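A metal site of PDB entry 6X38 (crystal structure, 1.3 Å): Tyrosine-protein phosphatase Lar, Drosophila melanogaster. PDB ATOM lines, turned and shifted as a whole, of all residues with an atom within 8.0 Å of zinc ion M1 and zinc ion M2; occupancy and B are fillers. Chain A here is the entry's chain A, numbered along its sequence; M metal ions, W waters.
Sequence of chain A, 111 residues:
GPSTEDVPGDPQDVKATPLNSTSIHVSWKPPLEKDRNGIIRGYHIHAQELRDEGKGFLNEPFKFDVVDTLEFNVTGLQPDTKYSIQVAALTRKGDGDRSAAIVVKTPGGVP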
ATOM      1  N   GLY A  42      30.647   1.705 -11.784  1.00  0.00           N
ATOM      2  CA  GLY A  42      29.854   0.614 -12.336  1.00  0.00           C
ATOM      3  C   GLY A  42      28.561   1.096 -12.931  1.00  0.00           C
ATOM      4  O   GLY A  42      27.871   1.960 -12.360  1.00  0.00           O
ATOM      5  N   TYR A  43      28.170   0.487 -14.055  1.00  0.00           N
ATOM      6  CA  TYR A  43      26.901   0.766 -14.716  1.00  0.00           C
ATOM      7  C   TYR A  43      26.274  -0.562 -15.154  1.00  0.00           C
ATOM      8  O   TYR A  43      26.956  -1.582 -15.319  1.00  0.00           O
ATOM      9  CB  TYR A  43      27.120   1.630 -16.017  1.00  0.00           C
ATOM     10  CG  TYR A  43      27.635   3.014 -15.686  1.00  0.00           C
ATOM     11  CD1 TYR A  43      28.994   3.252 -15.578  1.00  0.00           C
ATOM     12  CD2 TYR A  43      26.791   4.069 -15.577  1.00  0.00           C
ATOM     13  CE1 TYR A  43      29.478   4.532 -15.285  1.00  0.00           C
ATOM     14  CE2 TYR A  43      27.257   5.332 -15.262  1.00  0.00           C
ATOM     15  CZ  TYR A  43      28.598   5.559 -15.139  1.00  0.00           C
ATOM     16  OH  TYR A  43      29.024   6.871 -14.872  1.00  0.00           O
ATOM     17  N   HIS A  44      24.968  -0.525 -15.369  1.00  0.00           N
ATOM     18  CA  HIS A  44      24.237  -1.557 -16.120  1.00  0.00           C
ATOM     19  C   HIS A  44      23.817  -0.974 -17.474  1.00  0.00           C
ATOM     20  O   HIS A  44      23.368   0.180 -17.544  1.00  0.00           O
ATOM     21  CB  HIS A  44      22.962  -2.017 -15.444  1.00  0.00           C
ATOM     22  CG  HIS A  44      23.180  -2.971 -14.350  1.00  0.00           C
ATOM     23  ND1 HIS A  44      22.130  -3.358 -13.531  1.00  0.00           N
ATOM     24  CD2 HIS A  44      24.295  -3.640 -13.941  1.00  0.00           C
ATOM     25  CE1 HIS A  44      22.636  -4.259 -12.676  1.00  0.00           C
ATOM     26  NE2 HIS A  44      23.913  -4.449 -12.888  1.00  0.00           N
ATOM     27  N   ILE A  45      23.944  -1.779 -18.511  1.00  0.00           N
ATOM     28  CA  ILE A  45      23.213  -1.551 -19.769  1.00  0.00           C
ATOM     29  C   ILE A  45      22.096  -2.557 -19.823  1.00  0.00           C
ATOM     30  O   ILE A  45      22.327  -3.764 -19.709  1.00  0.00           O
ATOM     31  CB  ILE A  45      24.134  -1.646 -20.987  1.00  0.00           C
ATOM     32  CG1 ILE A  45      25.288  -0.664 -20.906  1.00  0.00           C
ATOM     33  CG2 ILE A  45      23.299  -1.457 -22.259  1.00  0.00           C
ATOM     34  CD1 ILE A  45      26.380  -0.977 -21.876  1.00  0.00           C
ATOM     35  N   HIS A  46      20.899  -2.065 -20.054  1.00  0.00           N
ATOM     36  CA  HIS A  46      19.709  -2.895 -20.163  1.00  0.00           C
ATOM     37  C   HIS A  46      19.247  -2.837 -21.609  1.00  0.00           C
ATOM     38  O   HIS A  46      19.064  -1.741 -22.140  1.00  0.00           O
ATOM     39  CB  HIS A  46      18.660  -2.397 -19.166  1.00  0.00           C
ATOM     40  CG  HIS A  46      18.963  -2.761 -17.725  1.00  0.00           C
ATOM     41  ND1 HIS A  46      18.708  -4.013 -17.236  1.00  0.00           N
ATOM     42  CD2 HIS A  46      19.452  -2.054 -16.671  1.00  0.00           C
ATOM     43  CE1 HIS A  46      19.049  -4.085 -15.955  1.00  0.00           C
ATOM     44  NE2 HIS A  46      19.492  -2.904 -15.594  1.00  0.00           N
ATOM     45  N   PHE A  62      18.135  -8.366 -21.842  1.00  0.00           N
ATOM     46  CA  PHE A  62      19.547  -8.563 -21.515  1.00  0.00           C
ATOM     47  C   PHE A  62      19.980  -7.501 -20.525  1.00  0.00           C
ATOM     48  O   PHE A  62      19.554  -6.326 -20.587  1.00  0.00           O
ATOM     49  CB  PHE A  62      20.424  -8.421 -22.785  1.00  0.00           C
ATOM     50  CG  PHE A  62      20.215  -9.458 -23.841  1.00  0.00           C
ATOM     51  CD1 PHE A  62      19.164  -9.351 -24.753  1.00  0.00           C
ATOM     52  CD2 PHE A  62      21.114 -10.500 -23.981  1.00  0.00           C
ATOM     53  CE1 PHE A  62      18.999 -10.323 -25.735  1.00  0.00           C
ATOM     54  CE2 PHE A  62      20.957 -11.468 -24.958  1.00  0.00           C
ATOM     55  CZ  PHE A  62      19.886 -11.372 -25.832  1.00  0.00           C
ATOM     56  N   LYS A  63      20.909  -7.871 -19.653  1.00  0.00           N
ATOM     57  CA  LYS A  63      21.590  -6.918 -18.780  1.00  0.00           C
ATOM     58  C   LYS A  63      23.066  -7.162 -18.892  1.00  0.00           C
ATOM     59  O   LYS A  63      23.512  -8.298 -18.912  1.00  0.00           O
ATOM     60  CB  LYS A  63      21.115  -7.127 -17.316  1.00  0.00           C
ATOM     61  CG  LYS A  63      21.763  -6.162 -16.309  1.00  0.00           C
ATOM     62  CD  LYS A  63      22.993  -6.725 -15.689  1.00  0.00           C
ATOM     63  CE  LYS A  63      22.601  -7.689 -14.580  1.00  0.00           C
ATOM     64  NZ  LYS A  63      23.697  -8.687 -14.258  1.00  0.00           N
ATOM     65  N   PHE A  64      23.828  -6.095 -18.937  1.00  0.00           N
ATOM     66  CA  PHE A  64      25.282  -6.147 -19.016  1.00  0.00           C
ATOM     67  C   PHE A  64      25.889  -5.318 -17.907  1.00  0.00           C
ATOM     68  O   PHE A  64      25.544  -4.144 -17.771  1.00  0.00           O
ATOM     69  CB  PHE A  64      25.772  -5.620 -20.378  1.00  0.00           C
ATOM     70  CG  PHE A  64      25.226  -6.411 -21.549  1.00  0.00           C
ATOM     71  CD1 PHE A  64      24.014  -6.090 -22.075  1.00  0.00           C
ATOM     72  CD2 PHE A  64      25.916  -7.477 -22.074  1.00  0.00           C
ATOM     73  CE1 PHE A  64      23.464  -6.819 -23.119  1.00  0.00           C
ATOM     74  CE2 PHE A  64      25.380  -8.213 -23.134  1.00  0.00           C
ATOM     75  CZ  PHE A  64      24.158  -7.855 -23.658  1.00  0.00           C
ATOM     76  N   ASP A  65      26.765  -5.902 -17.139  1.00  0.00           N
ATOM     77  CA  ASP A  65      27.536  -5.171 -16.154  1.00  0.00           C
ATOM     78  C   ASP A  65      28.759  -4.569 -16.766  1.00  0.00           C
ATOM     79  O   ASP A  65      29.505  -5.230 -17.500  1.00  0.00           O
ATOM     80  CB  ASP A  65      28.014  -6.088 -15.031  1.00  0.00           C
ATOM     81  CG  ASP A  65      26.945  -6.354 -14.080  1.00  0.00           C
ATOM     82  OD1 ASP A  65      26.811  -5.611 -13.056  1.00  0.00           O
ATOM     83  OD2 ASP A  65      26.175  -7.332 -14.277  1.00  0.00           O
ATOM     84  N   VAL A  66      28.994  -3.298 -16.503  1.00  0.00           N
ATOM     85  CA  VAL A  66      30.141  -2.536 -17.015  1.00  0.00           C
ATOM     86  C   VAL A  66      30.904  -2.000 -15.824  1.00  0.00           C
ATOM     87  O   VAL A  66      30.292  -1.480 -14.879  1.00  0.00           O
ATOM     88  CB  VAL A  66      29.644  -1.387 -17.929  1.00  0.00           C
ATOM     89  CG1 VAL A  66      30.839  -0.687 -18.649  1.00  0.00           C
ATOM     90  CG2 VAL A  66      28.663  -1.954 -18.980  1.00  0.00           C
ATOM     91  N   VAL A  67      32.207  -2.167 -15.819  1.00  0.00           N
ATOM     92  CA  VAL A  67      33.073  -1.657 -14.771  1.00  0.00           C
ATOM     93  C   VAL A  67      34.193  -0.839 -15.373  1.00  0.00           C
ATOM     94  O   VAL A  67      34.861  -1.297 -16.296  1.00  0.00           O
ATOM     95  CB  VAL A  67      33.671  -2.801 -13.924  1.00  0.00           C
ATOM     96  CG1 VAL A  67      34.640  -2.236 -12.916  1.00  0.00           C
ATOM     97  CG2 VAL A  67      32.552  -3.602 -13.243  1.00  0.00           C
ATOM     98  N   GLN A  86      18.979   1.222 -22.516  1.00  0.00           N
ATOM     99  CA  GLN A  86      19.049   2.161 -21.410  1.00  0.00           C
ATOM    100  C   GLN A  86      20.294   1.874 -20.592  1.00  0.00           C
ATOM    101  O   GLN A  86      20.701   0.714 -20.456  1.00  0.00           O
ATOM    102  CB  GLN A  86      17.776   2.084 -20.555  1.00  0.00           C
ATOM    103  CG  GLN A  86      16.538   2.568 -21.268  1.00  0.00           C
ATOM    104  CD  GLN A  86      15.318   2.551 -20.367  1.00  0.00           C
ATOM    105  OE1 GLN A  86      14.818   1.493 -20.056  1.00  0.00           O
ATOM    106  NE2 GLN A  86      14.876   3.692 -19.927  1.00  0.00           N
ATOM    107  N   VAL A  87      20.834   2.895 -19.951  1.00  0.00           N
ATOM    108  CA  VAL A  87      22.017   2.758 -19.101  1.00  0.00           C
ATOM    109  C   VAL A  87      21.641   3.319 -17.726  1.00  0.00           C
ATOM    110  O   VAL A  87      20.944   4.334 -17.632  1.00  0.00           O
ATOM    111  CB  VAL A  87      23.216   3.520 -19.706  1.00  0.00           C
ATOM    112  CG1 VAL A  87      24.479   3.243 -18.901  1.00  0.00           C
ATOM    113  CG2 VAL A  87      23.440   3.165 -21.167  1.00  0.00           C
ATOM    114  N   ALA A  88      22.191   2.701 -16.661  1.00  0.00           N
ATOM    115  CA  ALA A  88      21.957   3.176 -15.313  1.00  0.00           C
ATOM    116  C   ALA A  88      23.241   3.066 -14.513  1.00  0.00           C
ATOM    117  O   ALA A  88      23.959   2.069 -14.652  1.00  0.00           O
ATOM    118  CB  ALA A  88      20.852   2.390 -14.605  1.00  0.00           C
ATOM    119  N   ALA A  89      23.514   4.015 -13.644  1.00  0.00           N
ATOM    120  CA  ALA A  89      24.575   3.872 -12.655  1.00  0.00           C
ATOM    121  C   ALA A  89      24.157   2.929 -11.548  1.00  0.00           C
ATOM    122  O   ALA A  89      22.981   2.809 -11.241  1.00  0.00           O
ATOM    123  CB  ALA A  89      24.847   5.253 -12.037  1.00  0.00           C
ATOM    124  N   LEU A  90      25.125   2.270 -10.940  1.00  0.00           N
ATOM    125  CA  LEU A  90      24.847   1.362  -9.829  1.00  0.00           C
ATOM    126  C   LEU A  90      24.972   2.059  -8.505  1.00  0.00           C
ATOM    127  O   LEU A  90      25.907   2.813  -8.300  1.00  0.00           O
ATOM    128  CB  LEU A  90      25.798   0.164  -9.903  1.00  0.00           C
ATOM    129  CG  LEU A  90      25.627  -0.646 -11.197  1.00  0.00           C
ATOM    130  CD1 LEU A  90      26.614  -1.806 -11.298  1.00  0.00           C
ATOM    131  CD2 LEU A  90      24.218  -1.154 -11.363  1.00  0.00           C
ATOM    132  N   GLY A  94      20.208  -0.225  -5.647  1.00  0.00           N
ATOM    133  CA  GLY A  94      19.957  -0.769  -6.950  1.00  0.00           C
ATOM    134  C   GLY A  94      20.390   0.195  -8.038  1.00  0.00           C
ATOM    135  O   GLY A  94      21.330   1.000  -7.828  1.00  0.00           O
ATOM    136  N   ASP A  95      19.759   0.122  -9.168  1.00  0.00           N
ATOM    137  CA  ASP A  95      20.128   1.039 -10.240  1.00  0.00           C
ATOM    138  C   ASP A  95      19.657   2.447  -9.903  1.00  0.00           C
ATOM    139  O   ASP A  95      18.592   2.631  -9.303  1.00  0.00           O
ATOM    140  CB  ASP A  95      19.490   0.602 -11.560  1.00  0.00           C
ATOM    141  CG  ASP A  95      20.064  -0.706 -12.095  1.00  0.00           C
ATOM    142  OD1 ASP A  95      20.726  -1.488 -11.373  1.00  0.00           O
ATOM    143  OD2 ASP A  95      19.720  -1.058 -13.223  1.00  0.00           O
ATOM    144  N   GLY A  96      20.439   3.455 -10.315  1.00  0.00           N
ATOM    145  CA  GLY A  96      19.949   4.816 -10.356  1.00  0.00           C
ATOM    146  C   GLY A  96      19.030   4.958 -11.565  1.00  0.00           C
ATOM    147  O   GLY A  96      18.724   4.025 -12.284  1.00  0.00           O
ATOM    148  N   ARG A  98      17.420   5.377 -15.049  1.00  0.00           N
ATOM    149  CA  ARG A  98      17.845   4.965 -16.373  1.00  0.00           C
ATOM    150  C   ARG A  98      17.828   6.126 -17.352  1.00  0.00           C
ATOM    151  O   ARG A  98      16.957   6.988 -17.285  1.00  0.00           O
ATOM    152  CB  ARG A  98      16.923   3.878 -16.922  1.00  0.00           C
ATOM    153  CG  ARG A  98      16.959   2.589 -16.146  1.00  0.00           C
ATOM    154  CD  ARG A  98      16.091   1.572 -16.874  1.00  0.00           C
ATOM    155  NE  ARG A  98      16.175   0.250 -16.272  1.00  0.00           N
ATOM    156  CZ  ARG A  98      15.836  -0.878 -16.906  1.00  0.00           C
ATOM    157  NH1 ARG A  98      15.453  -0.853 -18.182  1.00  0.00           N
ATOM    158  NH2 ARG A  98      15.967  -2.017 -16.264  1.00  0.00           N
HETATM  159 ZN    ZN M   1      20.261  -2.819 -13.714  1.00  0.00          ZN
HETATM  160 ZN    ZN M   2      25.152  -5.723 -11.955  1.00  0.00          ZN
HETATM  161  O   HOH W   1      19.245  -4.079 -12.473  1.00  0.00           O
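The backbone carbonyl oxygen (O) of Ala 88 sits at hydrogen-bond distance from the backbone NH (N) of His 44 (2.9 Å).
OD2 of Asp 65 is in salt-bridge range of NZ of Lys 63 (2.8 Å).
The backbone carbonyl oxygen (O) of Gln 86 is in hydrogen-bond range of the backbone NH (N) of His 46.
Within 4 Å of zinc ion M1: His 44, His 46 and Asp 95.
Of the 20 residues printed, 2 come within 4 Å of zinc ion M2.
Zinc ion M1 is bound by the side-chain carboxylate (OD2) of Asp 95 (1.9 Å), a ring nitrogen (ND1) of His 44 (2.0 Å), a ring nitrogen (NE2) of His 46 (2.0 Å) and water W1 (2.0 Å).
Slightly farther from zinc ion M1 lies OD1 of Asp 95 (2.7 Å).
Zinc ion M2 is bound by the side-chain carboxylate of Asp 65 (2.0 Å) and a ring nitrogen (NE2) of His 44 (2.0 Å).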
